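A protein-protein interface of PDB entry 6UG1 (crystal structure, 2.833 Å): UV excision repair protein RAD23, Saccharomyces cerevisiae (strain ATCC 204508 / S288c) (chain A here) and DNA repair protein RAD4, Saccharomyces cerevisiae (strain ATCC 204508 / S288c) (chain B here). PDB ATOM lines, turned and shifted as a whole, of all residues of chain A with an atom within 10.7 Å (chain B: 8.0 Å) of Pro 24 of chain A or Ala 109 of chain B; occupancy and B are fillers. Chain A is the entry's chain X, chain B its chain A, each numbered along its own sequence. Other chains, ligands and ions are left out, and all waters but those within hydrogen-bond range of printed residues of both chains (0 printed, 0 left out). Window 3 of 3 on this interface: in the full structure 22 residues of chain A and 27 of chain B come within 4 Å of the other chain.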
ATOM      1  N   ASP A   7      -4.198  -5.334 -17.771  1.00  0.00           N
ATOM      2  CA  ASP A   7      -2.790  -5.052 -17.916  1.00  0.00           C
ATOM      3  C   ASP A   7      -1.993  -5.764 -16.847  1.00  0.00           C
ATOM      4  O   ASP A   7      -0.984  -6.398 -17.163  1.00  0.00           O
ATOM      5  CB  ASP A   7      -2.557  -3.538 -17.782  1.00  0.00           C
ATOM      6  CG  ASP A   7      -3.211  -2.731 -18.879  1.00  0.00           C
ATOM      7  OD1 ASP A   7      -3.361  -3.311 -19.973  1.00  0.00           O
ATOM      8  OD2 ASP A   7      -3.540  -1.530 -18.659  1.00  0.00           O
ATOM      9  N   SER A  10      -1.608  -9.378 -18.142  1.00  0.00           N
ATOM     10  CA  SER A  10      -0.688  -9.579 -19.264  1.00  0.00           C
ATOM     11  C   SER A  10       0.738  -9.338 -18.809  1.00  0.00           C
ATOM     12  O   SER A  10       1.674  -9.987 -19.312  1.00  0.00           O
ATOM     13  CB  SER A  10      -1.050  -8.714 -20.493  1.00  0.00           C
ATOM     14  OG  SER A  10      -1.573  -7.465 -20.141  1.00  0.00           O
ATOM     15  N   LEU A  11       0.919  -8.455 -17.822  1.00  0.00           N
ATOM     16  CA  LEU A  11       2.262  -8.107 -17.433  1.00  0.00           C
ATOM     17  C   LEU A  11       2.853  -9.230 -16.582  1.00  0.00           C
ATOM     18  O   LEU A  11       3.982  -9.683 -16.829  1.00  0.00           O
ATOM     19  CB  LEU A  11       2.255  -6.867 -16.540  1.00  0.00           C
ATOM     20  CG  LEU A  11       3.663  -6.290 -16.243  1.00  0.00           C
ATOM     21  CD1 LEU A  11       4.272  -5.878 -17.599  1.00  0.00           C
ATOM     22  CD2 LEU A  11       3.812  -5.258 -15.216  1.00  0.00           C
ATOM     23  N   VAL A  14       3.856 -11.943 -19.217  1.00  0.00           N
ATOM     24  CA  VAL A  14       5.144 -11.677 -19.867  1.00  0.00           C
ATOM     25  C   VAL A  14       6.292 -11.871 -18.873  1.00  0.00           C
ATOM     26  O   VAL A  14       7.356 -12.428 -19.188  1.00  0.00           O
ATOM     27  CB  VAL A  14       5.211 -10.291 -20.480  1.00  0.00           C
ATOM     28  CG1 VAL A  14       6.609 -10.039 -20.795  1.00  0.00           C
ATOM     29  CG2 VAL A  14       4.365 -10.234 -21.708  1.00  0.00           C
ATOM     30  N   ASN A  18       7.841 -14.855 -20.728  1.00  0.00           N
ATOM     31  CA  ASN A  18       8.514 -14.303 -21.899  1.00  0.00           C
ATOM     32  C   ASN A  18       9.158 -12.971 -21.572  1.00  0.00           C
ATOM     33  O   ASN A  18       8.795 -11.949 -22.156  1.00  0.00           O
ATOM     34  CB  ASN A  18       7.546 -14.133 -23.071  1.00  0.00           C
ATOM     35  CG  ASN A  18       6.987 -15.439 -23.574  1.00  0.00           C
ATOM     36  OD1 ASN A  18       5.929 -15.912 -23.142  1.00  0.00           O
ATOM     37  ND2 ASN A  18       7.726 -16.058 -24.488  1.00  0.00           N
ATOM     38  N   PRO A  19      10.096 -12.919 -20.611  1.00  0.00           N
ATOM     39  CA  PRO A  19      10.625 -11.590 -20.223  1.00  0.00           C
ATOM     40  C   PRO A  19      11.494 -10.944 -21.279  1.00  0.00           C
ATOM     41  O   PRO A  19      11.656  -9.722 -21.253  1.00  0.00           O
ATOM     42  CB  PRO A  19      11.367 -11.858 -18.914  1.00  0.00           C
ATOM     43  CG  PRO A  19      11.658 -13.295 -18.920  1.00  0.00           C
ATOM     44  CD  PRO A  19      10.571 -13.981 -19.712  1.00  0.00           C
ATOM     45  N   GLU A  20      12.010 -11.700 -22.235  1.00  0.00           N
ATOM     46  CA  GLU A  20      12.700 -11.096 -23.379  1.00  0.00           C
ATOM     47  C   GLU A  20      11.834  -9.999 -24.019  1.00  0.00           C
ATOM     48  O   GLU A  20      12.366  -8.994 -24.505  1.00  0.00           O
ATOM     49  CB  GLU A  20      13.089 -12.156 -24.411  1.00  0.00           C
ATOM     50  CG  GLU A  20      11.904 -13.112 -24.807  1.00  0.00           C
ATOM     51  CD  GLU A  20      11.599 -14.296 -23.839  1.00  0.00           C
ATOM     52  OE1 GLU A  20      12.082 -14.340 -22.684  1.00  0.00           O
ATOM     53  OE2 GLU A  20      10.849 -15.202 -24.261  1.00  0.00           O
ATOM     54  N   ALA A  21      10.499 -10.219 -24.091  1.00  0.00           N
ATOM     55  CA  ALA A  21       9.492  -9.317 -24.701  1.00  0.00           C
ATOM     56  C   ALA A  21       8.955  -8.220 -23.791  1.00  0.00           C
ATOM     57  O   ALA A  21       8.089  -7.466 -24.231  1.00  0.00           O
ATOM     58  CB  ALA A  21       8.239 -10.091 -25.202  1.00  0.00           C
ATOM     59  N   LEU A  22       9.455  -8.095 -22.564  1.00  0.00           N
ATOM     60  CA  LEU A  22       9.078  -7.002 -21.650  1.00  0.00           C
ATOM     61  C   LEU A  22       9.115  -5.606 -22.269  1.00  0.00           C
ATOM     62  O   LEU A  22       8.154  -4.851 -22.161  1.00  0.00           O
ATOM     63  CB  LEU A  22       9.987  -7.074 -20.425  1.00  0.00           C
ATOM     64  CG  LEU A  22       9.315  -7.856 -19.305  1.00  0.00           C
ATOM     65  CD1 LEU A  22      10.203  -8.095 -18.109  1.00  0.00           C
ATOM     66  CD2 LEU A  22       8.201  -7.010 -18.804  1.00  0.00           C
ATOM     67  N   ALA A  23      10.164  -5.268 -22.962  1.00  0.00           N
ATOM     68  CA  ALA A  23      10.448  -3.885 -23.344  1.00  0.00           C
ATOM     69  C   ALA A  23       9.292  -3.081 -23.936  1.00  0.00           C
ATOM     70  O   ALA A  23       8.956  -2.019 -23.383  1.00  0.00           O
ATOM     71  CB  ALA A  23      11.612  -3.858 -24.335  1.00  0.00           C
ATOM     72  N   PRO A  24       8.662  -3.509 -25.031  1.00  0.00           N
ATOM     73  CA  PRO A  24       7.544  -2.699 -25.566  1.00  0.00           C
ATOM     74  C   PRO A  24       6.312  -2.631 -24.665  1.00  0.00           C
ATOM     75  O   PRO A  24       5.756  -1.530 -24.508  1.00  0.00           O
ATOM     76  CB  PRO A  24       7.218  -3.416 -26.886  1.00  0.00           C
ATOM     77  CG  PRO A  24       7.684  -4.870 -26.647  1.00  0.00           C
ATOM     78  CD  PRO A  24       8.926  -4.722 -25.826  1.00  0.00           C
ATOM     79  N   LEU A  25       6.017  -3.682 -23.888  1.00  0.00           N
ATOM     80  CA  LEU A  25       4.842  -3.638 -23.039  1.00  0.00           C
ATOM     81  C   LEU A  25       5.026  -2.549 -21.988  1.00  0.00           C
ATOM     82  O   LEU A  25       4.142  -1.700 -21.791  1.00  0.00           O
ATOM     83  CB  LEU A  25       4.615  -5.001 -22.400  1.00  0.00           C
ATOM     84  CG  LEU A  25       3.537  -5.069 -21.314  1.00  0.00           C
ATOM     85  CD1 LEU A  25       2.277  -4.384 -21.900  1.00  0.00           C
ATOM     86  CD2 LEU A  25       3.267  -6.530 -20.891  1.00  0.00           C
ATOM     87  N   LEU A  26       6.224  -2.501 -21.382  1.00  0.00           N
ATOM     88  CA  LEU A  26       6.533  -1.533 -20.324  1.00  0.00           C
ATOM     89  C   LEU A  26       6.548  -0.125 -20.861  1.00  0.00           C
ATOM     90  O   LEU A  26       6.176   0.822 -20.153  1.00  0.00           O
ATOM     91  CB  LEU A  26       7.909  -1.775 -19.719  1.00  0.00           C
ATOM     92  CG  LEU A  26       8.262  -2.998 -18.902  1.00  0.00           C
ATOM     93  CD1 LEU A  26       9.698  -2.815 -18.465  1.00  0.00           C
ATOM     94  CD2 LEU A  26       7.330  -3.095 -17.698  1.00  0.00           C
ATOM     95  N   GLU A  27       7.041   0.024 -22.089  1.00  0.00           N
ATOM     96  CA  GLU A  27       6.976   1.306 -22.756  1.00  0.00           C
ATOM     97  C   GLU A  27       5.509   1.752 -22.824  1.00  0.00           C
ATOM     98  O   GLU A  27       5.105   2.739 -22.197  1.00  0.00           O
ATOM     99  CB  GLU A  27       7.597   1.143 -24.143  1.00  0.00           C
ATOM    100  CG  GLU A  27       7.848   2.416 -24.933  1.00  0.00           C
ATOM    101  CD  GLU A  27       9.131   3.030 -24.463  1.00  0.00           C
ATOM    102  OE1 GLU A  27      10.099   2.239 -24.231  1.00  0.00           O
ATOM    103  OE2 GLU A  27       9.160   4.273 -24.319  1.00  0.00           O
ATOM    104  N   ASN A  28       4.666   0.902 -23.424  1.00  0.00           N
ATOM    105  CA  ASN A  28       3.228   1.153 -23.500  1.00  0.00           C
ATOM    106  C   ASN A  28       2.654   1.517 -22.135  1.00  0.00           C
ATOM    107  O   ASN A  28       2.022   2.566 -21.967  1.00  0.00           O
ATOM    108  CB  ASN A  28       2.521  -0.047 -24.119  1.00  0.00           C
ATOM    109  CG  ASN A  28       1.057  -0.003 -23.882  1.00  0.00           C
ATOM    110  OD1 ASN A  28       0.582  -0.515 -22.872  1.00  0.00           O
ATOM    111  ND2 ASN A  28       0.335   0.744 -24.728  1.00  0.00           N
ATOM    112  N   ILE A  29       2.696   0.585 -21.204  1.00  0.00           N
ATOM    113  CA  ILE A  29       1.998   0.793 -19.955  1.00  0.00           C
ATOM    114  C   ILE A  29       2.561   2.037 -19.281  1.00  0.00           C
ATOM    115  O   ILE A  29       1.822   2.840 -18.708  1.00  0.00           O
ATOM    116  CB  ILE A  29       2.200  -0.432 -19.065  1.00  0.00           C
ATOM    117  CG1 ILE A  29       1.376  -0.400 -17.803  1.00  0.00           C
ATOM    118  CG2 ILE A  29       3.581  -0.417 -18.539  1.00  0.00           C
ATOM    119  CD1 ILE A  29       1.271  -1.868 -17.175  1.00  0.00           C
ATOM    120  N   SER A  30       3.878   2.252 -19.361  1.00  0.00           N
ATOM    121  CA  SER A  30       4.377   3.453 -18.688  1.00  0.00           C
ATOM    122  C   SER A  30       3.821   4.705 -19.365  1.00  0.00           C
ATOM    123  O   SER A  30       3.636   5.732 -18.706  1.00  0.00           O
ATOM    124  CB  SER A  30       5.915   3.504 -18.639  1.00  0.00           C
ATOM    125  OG  SER A  30       6.457   3.828 -19.909  1.00  0.00           O
ATOM    126  N   ALA A  31       3.604   4.647 -20.687  1.00  0.00           N
ATOM    127  CA  ALA A  31       2.948   5.723 -21.416  1.00  0.00           C
ATOM    128  C   ALA A  31       1.466   5.831 -21.097  1.00  0.00           C
ATOM    129  O   ALA A  31       0.885   6.910 -21.266  1.00  0.00           O
ATOM    130  CB  ALA A  31       3.112   5.514 -22.915  1.00  0.00           C
ATOM    131  N   ARG A  32       0.838   4.769 -20.607  1.00  0.00           N
ATOM    132  CA  ARG A  32      -0.560   4.881 -20.238  1.00  0.00           C
ATOM    133  C   ARG A  32      -0.780   5.123 -18.760  1.00  0.00           C
ATOM    134  O   ARG A  32      -1.929   5.303 -18.353  1.00  0.00           O
ATOM    135  CB  ARG A  32      -1.359   3.664 -20.691  1.00  0.00           C
ATOM    136  CG  ARG A  32      -1.609   3.680 -22.197  1.00  0.00           C
ATOM    137  CD  ARG A  32      -2.734   2.755 -22.603  1.00  0.00           C
ATOM    138  NE  ARG A  32      -2.353   1.350 -22.526  1.00  0.00           N
ATOM    139  CZ  ARG A  32      -2.662   0.516 -21.526  1.00  0.00           C
ATOM    140  NH1 ARG A  32      -3.366   0.930 -20.479  1.00  0.00           N
ATOM    141  NH2 ARG A  32      -2.257  -0.754 -21.573  1.00  0.00           N
ATOM    142  N   LEU A  36       2.341   5.711 -12.355  1.00  0.00           N
ATOM    143  CA  LEU A  36       3.093   4.493 -12.027  1.00  0.00           C
ATOM    144  C   LEU A  36       4.567   4.774 -11.723  1.00  0.00           C
ATOM    145  O   LEU A  36       5.096   4.325 -10.697  1.00  0.00           O
ATOM    146  CB  LEU A  36       2.968   3.472 -13.161  1.00  0.00           C
ATOM    147  CG  LEU A  36       3.991   2.359 -13.165  1.00  0.00           C
ATOM    148  CD1 LEU A  36       3.462   1.460 -12.041  1.00  0.00           C
ATOM    149  CD2 LEU A  36       4.032   1.681 -14.487  1.00  0.00           C
ATOM    150  N   PHE B  15      13.773   3.536 -15.683  1.00  0.00           N
ATOM    151  CA  PHE B  15      13.459   2.379 -16.483  1.00  0.00           C
ATOM    152  C   PHE B  15      14.360   1.228 -16.043  1.00  0.00           C
ATOM    153  O   PHE B  15      13.947   0.070 -16.098  1.00  0.00           O
ATOM    154  CB  PHE B  15      13.656   2.762 -17.934  1.00  0.00           C
ATOM    155  CG  PHE B  15      12.865   1.964 -18.860  1.00  0.00           C
ATOM    156  CD1 PHE B  15      13.370   0.808 -19.422  1.00  0.00           C
ATOM    157  CD2 PHE B  15      11.622   2.458 -19.261  1.00  0.00           C
ATOM    158  CE1 PHE B  15      12.620   0.089 -20.310  1.00  0.00           C
ATOM    159  CE2 PHE B  15      10.869   1.794 -20.137  1.00  0.00           C
ATOM    160  CZ  PHE B  15      11.358   0.586 -20.691  1.00  0.00           C
ATOM    161  N   TYR B  19      12.820  -2.322 -14.969  1.00  0.00           N
ATOM    162  CA  TYR B  19      13.280  -3.505 -15.671  1.00  0.00           C
ATOM    163  C   TYR B  19      13.922  -4.463 -14.662  1.00  0.00           C
ATOM    164  O   TYR B  19      13.719  -5.687 -14.700  1.00  0.00           O
ATOM    165  CB  TYR B  19      14.190  -2.979 -16.748  1.00  0.00           C
ATOM    166  CG  TYR B  19      14.349  -3.833 -17.863  1.00  0.00           C
ATOM    167  CD1 TYR B  19      15.016  -5.032 -17.732  1.00  0.00           C
ATOM    168  CD2 TYR B  19      13.779  -3.456 -19.112  1.00  0.00           C
ATOM    169  CE1 TYR B  19      15.167  -5.894 -18.839  1.00  0.00           C
ATOM    170  CE2 TYR B  19      13.909  -4.284 -20.230  1.00  0.00           C
ATOM    171  CZ  TYR B  19      14.622  -5.528 -20.072  1.00  0.00           C
ATOM    172  OH  TYR B  19      14.836  -6.425 -21.095  1.00  0.00           O
ATOM    173  N   ARG B 100      21.056  -5.573 -22.824  1.00  0.00           N
ATOM    174  CA  ARG B 100      20.740  -4.856 -24.068  1.00  0.00           C
ATOM    175  C   ARG B 100      21.083  -3.369 -23.995  1.00  0.00           C
ATOM    176  O   ARG B 100      21.229  -2.785 -22.910  1.00  0.00           O
ATOM    177  CB  ARG B 100      19.270  -5.016 -24.464  1.00  0.00           C
ATOM    178  CG  ARG B 100      18.886  -6.347 -25.172  1.00  0.00           C
ATOM    179  CD  ARG B 100      17.395  -6.687 -24.959  1.00  0.00           C
ATOM    180  NE  ARG B 100      17.053  -7.970 -25.564  1.00  0.00           N
ATOM    181  CZ  ARG B 100      15.816  -8.421 -25.723  1.00  0.00           C
ATOM    182  NH1 ARG B 100      14.776  -7.684 -25.315  1.00  0.00           N
ATOM    183  NH2 ARG B 100      15.632  -9.629 -26.289  1.00  0.00           N
ATOM    184  N   TRP B 102      20.457   0.721 -24.890  1.00  0.00           N
ATOM    185  CA  TRP B 102      19.343   1.653 -24.922  1.00  0.00           C
ATOM    186  C   TRP B 102      18.788   1.734 -26.328  1.00  0.00           C
ATOM    187  O   TRP B 102      17.574   1.881 -26.518  1.00  0.00           O
ATOM    188  CB  TRP B 102      19.752   3.015 -24.384  1.00  0.00           C
ATOM    189  CG  TRP B 102      20.029   2.946 -22.919  1.00  0.00           C
ATOM    190  CD1 TRP B 102      21.234   3.046 -22.332  1.00  0.00           C
ATOM    191  CD2 TRP B 102      19.073   2.725 -21.843  1.00  0.00           C
ATOM    192  NE1 TRP B 102      21.120   2.899 -20.963  1.00  0.00           N
ATOM    193  CE2 TRP B 102      19.804   2.705 -20.640  1.00  0.00           C
ATOM    194  CE3 TRP B 102      17.671   2.560 -21.782  1.00  0.00           C
ATOM    195  CZ2 TRP B 102      19.194   2.508 -19.380  1.00  0.00           C
ATOM    196  CZ3 TRP B 102      17.055   2.376 -20.499  1.00  0.00           C
ATOM    197  CH2 TRP B 102      17.817   2.341 -19.336  1.00  0.00           C
ATOM    198  N   LYS B 103      19.659   1.772 -27.327  1.00  0.00           N
ATOM    199  CA  LYS B 103      19.149   1.812 -28.684  1.00  0.00           C
ATOM    200  C   LYS B 103      18.330   0.549 -28.940  1.00  0.00           C
ATOM    201  O   LYS B 103      17.247   0.610 -29.526  1.00  0.00           O
ATOM    202  CB  LYS B 103      20.302   1.972 -29.690  1.00  0.00           C
ATOM    203  CG  LYS B 103      19.878   2.406 -31.130  1.00  0.00           C
ATOM    204  CD  LYS B 103      21.096   2.744 -32.031  1.00  0.00           C
ATOM    205  CE  LYS B 103      22.355   1.842 -31.803  1.00  0.00           C
ATOM    206  NZ  LYS B 103      23.414   2.255 -32.770  1.00  0.00           N
ATOM    207  N   GLU B 104      18.867  -0.622 -28.558  1.00  0.00           N
ATOM    208  CA  GLU B 104      18.166  -1.883 -28.825  1.00  0.00           C
ATOM    209  C   GLU B 104      16.772  -1.884 -28.204  1.00  0.00           C
ATOM    210  O   GLU B 104      15.774  -2.123 -28.891  1.00  0.00           O
ATOM    211  CB  GLU B 104      19.010  -3.070 -28.324  1.00  0.00           C
ATOM    212  CG  GLU B 104      20.179  -3.447 -29.286  1.00  0.00           C
ATOM    213  CD  GLU B 104      21.143  -4.445 -28.678  1.00  0.00           C
ATOM    214  OE1 GLU B 104      20.877  -4.877 -27.529  1.00  0.00           O
ATOM    215  OE2 GLU B 104      22.188  -4.751 -29.314  1.00  0.00           O
ATOM    216  N   ILE B 105      16.680  -1.532 -26.919  1.00  0.00           N
ATOM    217  CA  ILE B 105      15.375  -1.328 -26.267  1.00  0.00           C
ATOM    218  C   ILE B 105      14.473  -0.392 -27.047  1.00  0.00           C
ATOM    219  O   ILE B 105      13.326  -0.726 -27.348  1.00  0.00           O
ATOM    220  CB  ILE B 105      15.537  -0.866 -24.813  1.00  0.00           C
ATOM    221  CG1 ILE B 105      16.512  -1.841 -24.104  1.00  0.00           C
ATOM    222  CG2 ILE B 105      14.112  -0.642 -24.154  1.00  0.00           C
ATOM    223  CD1 ILE B 105      16.802  -1.515 -22.703  1.00  0.00           C
ATOM    224  N   GLU B 106      14.881   0.859 -27.187  1.00  0.00           N
ATOM    225  CA  GLU B 106      14.002   1.809 -27.851  1.00  0.00           C
ATOM    226  C   GLU B 106      13.438   1.149 -29.104  1.00  0.00           C
ATOM    227  O   GLU B 106      12.211   1.120 -29.325  1.00  0.00           O
ATOM    228  CB  GLU B 106      14.794   3.084 -28.211  1.00  0.00           C
ATOM    229  CG  GLU B 106      14.083   4.131 -29.040  1.00  0.00           C
ATOM    230  CD  GLU B 106      15.020   5.278 -29.522  1.00  0.00           C
ATOM    231  OE1 GLU B 106      16.220   5.013 -29.789  1.00  0.00           O
ATOM    232  OE2 GLU B 106      14.558   6.439 -29.673  1.00  0.00           O
ATOM    233  N   MET B 107      14.322   0.495 -29.881  1.00  0.00           N
ATOM    234  CA  MET B 107      13.823  -0.095 -31.105  1.00  0.00           C
ATOM    235  C   MET B 107      12.937  -1.320 -30.854  1.00  0.00           C
ATOM    236  O   MET B 107      12.158  -1.677 -31.746  1.00  0.00           O
ATOM    237  CB  MET B 107      15.057  -0.530 -31.953  1.00  0.00           C
ATOM    238  CG  MET B 107      16.065   0.587 -32.444  1.00  0.00           C
ATOM    239  SD  MET B 107      15.476   2.102 -33.270  1.00  0.00           S
ATOM    240  CE  MET B 107      16.947   3.146 -33.340  1.00  0.00           C
ATOM    241  N   SER B 108      12.991  -1.971 -29.672  1.00  0.00           N
ATOM    242  CA  SER B 108      12.129  -3.150 -29.575  1.00  0.00           C
ATOM    243  C   SER B 108      10.736  -2.690 -29.181  1.00  0.00           C
ATOM    244  O   SER B 108       9.731  -3.247 -29.639  1.00  0.00           O
ATOM    245  CB  SER B 108      12.633  -4.164 -28.544  1.00  0.00           C
ATOM    246  OG  SER B 108      12.141  -3.848 -27.253  1.00  0.00           O
ATOM    247  N   ALA B 109      10.709  -1.560 -28.452  1.00  0.00           N
ATOM    248  CA  ALA B 109       9.498  -0.812 -28.109  1.00  0.00           C
ATOM    249  C   ALA B 109       8.733  -0.532 -29.371  1.00  0.00           C
ATOM    250  O   ALA B 109       7.568  -0.916 -29.540  1.00  0.00           O
ATOM    251  CB  ALA B 109       9.830   0.468 -27.357  1.00  0.00           C
ATOM    252  N   ASN B 110       9.436   0.095 -30.305  1.00  0.00           N
ATOM    253  CA  ASN B 110       8.908   0.552 -31.586  1.00  0.00           C
ATOM    254  C   ASN B 110       8.223  -0.647 -32.238  1.00  0.00           C
ATOM    255  O   ASN B 110       7.015  -0.581 -32.470  1.00  0.00           O
ATOM    256  CB  ASN B 110      10.040   1.059 -32.488  1.00  0.00           C
ATOM    257  CG  ASN B 110       9.628   2.185 -33.421  1.00  0.00           C
ATOM    258  OD1 ASN B 110       8.442   2.456 -33.544  1.00  0.00           O
ATOM    259  ND2 ASN B 110      10.542   2.488 -34.330  1.00  0.00           N
ATOM    260  N   ASN B 111       8.986  -1.657 -32.677  1.00  0.00           N
ATOM    261  CA  ASN B 111       8.435  -2.866 -33.319  1.00  0.00           C
ATOM    262  C   ASN B 111       7.800  -3.857 -32.342  1.00  0.00           C
ATOM    263  O   ASN B 111       8.502  -4.565 -31.607  1.00  0.00           O
ATOM    264  CB  ASN B 111       9.526  -3.557 -34.125  1.00  0.00           C
ATOM    265  CG  ASN B 111       9.805  -2.815 -35.408  1.00  0.00           C
ATOM    266  OD1 ASN B 111      10.645  -1.913 -35.439  1.00  0.00           O
ATOM    267  ND2 ASN B 111       9.061  -3.140 -36.468  1.00  0.00           N
ATOM    268  N   LYS B 112       6.457  -3.978 -32.463  1.00  0.00           N
ATOM    269  CA  LYS B 112       5.576  -4.831 -31.663  1.00  0.00           C
ATOM    270  C   LYS B 112       5.468  -6.301 -32.073  1.00  0.00           C
ATOM    271  O   LYS B 112       5.363  -7.176 -31.203  1.00  0.00           O
ATOM    272  CB  LYS B 112       4.159  -4.297 -31.755  1.00  0.00           C
ATOM    273  CG  LYS B 112       3.951  -2.823 -31.549  1.00  0.00           C
ATOM    274  CD  LYS B 112       2.442  -2.595 -31.491  1.00  0.00           C
ATOM    275  CE  LYS B 112       2.043  -1.151 -31.269  1.00  0.00           C
ATOM    276  NZ  LYS B 112       0.543  -0.975 -31.287  1.00  0.00           N
ATOM    277  N   ARG B 113       5.414  -6.597 -33.362  1.00  0.00           N
ATOM    278  CA  ARG B 113       5.524  -7.965 -33.879  1.00  0.00           C
ATOM    279  C   ARG B 113       4.516  -8.896 -33.184  1.00  0.00           C
ATOM    280  O   ARG B 113       3.416  -8.486 -32.806  1.00  0.00           O
ATOM    281  CB  ARG B 113       6.960  -8.421 -33.738  1.00  0.00           C
ATOM    282  CG  ARG B 113       7.915  -7.676 -34.575  1.00  0.00           C
ATOM    283  CD  ARG B 113       7.772  -8.148 -35.985  1.00  0.00           C
ATOM    284  NE  ARG B 113       8.661  -7.416 -36.875  1.00  0.00           N
ATOM    285  CZ  ARG B 113       8.358  -6.262 -37.457  1.00  0.00           C
ATOM    286  NH1 ARG B 113       7.173  -5.695 -37.248  1.00  0.00           N
ATOM    287  NH2 ARG B 113       9.242  -5.683 -38.257  1.00  0.00           N
ATOM    288  N   PHE B 115       4.425 -12.376 -30.393  1.00  0.00           N
ATOM    289  CA  PHE B 115       5.263 -13.020 -29.383  1.00  0.00           C
ATOM    290  C   PHE B 115       4.448 -14.172 -28.836  1.00  0.00           C
ATOM    291  O   PHE B 115       3.315 -13.999 -28.376  1.00  0.00           O
ATOM    292  CB  PHE B 115       5.713 -12.174 -28.184  1.00  0.00           C
ATOM    293  CG  PHE B 115       4.598 -11.601 -27.378  1.00  0.00           C
ATOM    294  CD1 PHE B 115       3.510 -10.958 -27.957  1.00  0.00           C
ATOM    295  CD2 PHE B 115       4.562 -11.885 -26.011  1.00  0.00           C
ATOM    296  CE1 PHE B 115       2.466 -10.494 -27.170  1.00  0.00           C
ATOM    297  CE2 PHE B 115       3.520 -11.444 -25.231  1.00  0.00           C
ATOM    298  CZ  PHE B 115       2.468 -10.750 -25.807  1.00  0.00           C
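O of Glu 20 of chain A lies within hydrogen-bond range of NH1 of Arg 100 of chain B (2.9 Å).
The side-chain hydroxyl of Ser 108 of chain B sits at hydrogen-bond distance from the backbone carbonyl oxygen of Ile 105 of chain B (3.3 Å).
ND2 of Asn 18 of chain A lies within hydrogen-bond range of OE2 of Glu 20 of chain A (3.2 Å).
The side-chain hydroxyl (OG) of Ser 30 of chain A lies within hydrogen-bond range of the backbone carbonyl oxygen (O) of Glu 27 of chain A, at 2.9 Å.
Val 14 of chain A touches Phe 115 of chain B (CG2 to CE2, 3.8 Å).
Ala 23 of chain A touches Ser 108 of chain B (CB to OG, 3.0 Å).
Pro 24 of chain A touches Ser 108 of chain B (CD to OG, 3.6 Å).
CB of Pro 24 of chain A touches O of Ala 109 of chain B, at 3.7 Å.
OE1 of Glu 27 of chain A touches CB of Ala 109 of chain B, at 3.6 Å.
Pro 24 of chain A touches just these residues of chain B: Ser 108 (3.6 Å) and Ala 109 (3.7 Å).
Of the printed residues of chain A, Ala 109 of chain B touches Pro 24 and Glu 27.
Printed residues of chain B within 4 Å of Ala 23 of chain A: Ser 108.
Ser 108 of chain B touches two residues of chain A.
Printed residues of chain B within 4 Å of Glu 27 of chain A: Ala 109 (3.6 Å).
Printed residues of chain A within 4 Å of Phe 115 of chain B: Val 14 (3.8 Å).
Of the printed residues of chain A, Arg 100 of chain B touches Glu 20.
Of the printed residues of chain B, Glu 20 of chain A touches Arg 100.
Tyr 19 of chain B touches none of the printed residues of chain A.
The nearest residue of chain A that does not touch Ala 109 of chain B is Ala 23 of chain A (4.8 Å).
Among the printed residues, 6 pairs touch across the chains.
Among the printed residues, no Asp or Glu carboxylate lies within 4 Å of a Lys or Arg side-chain nitrogen of the other chain.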
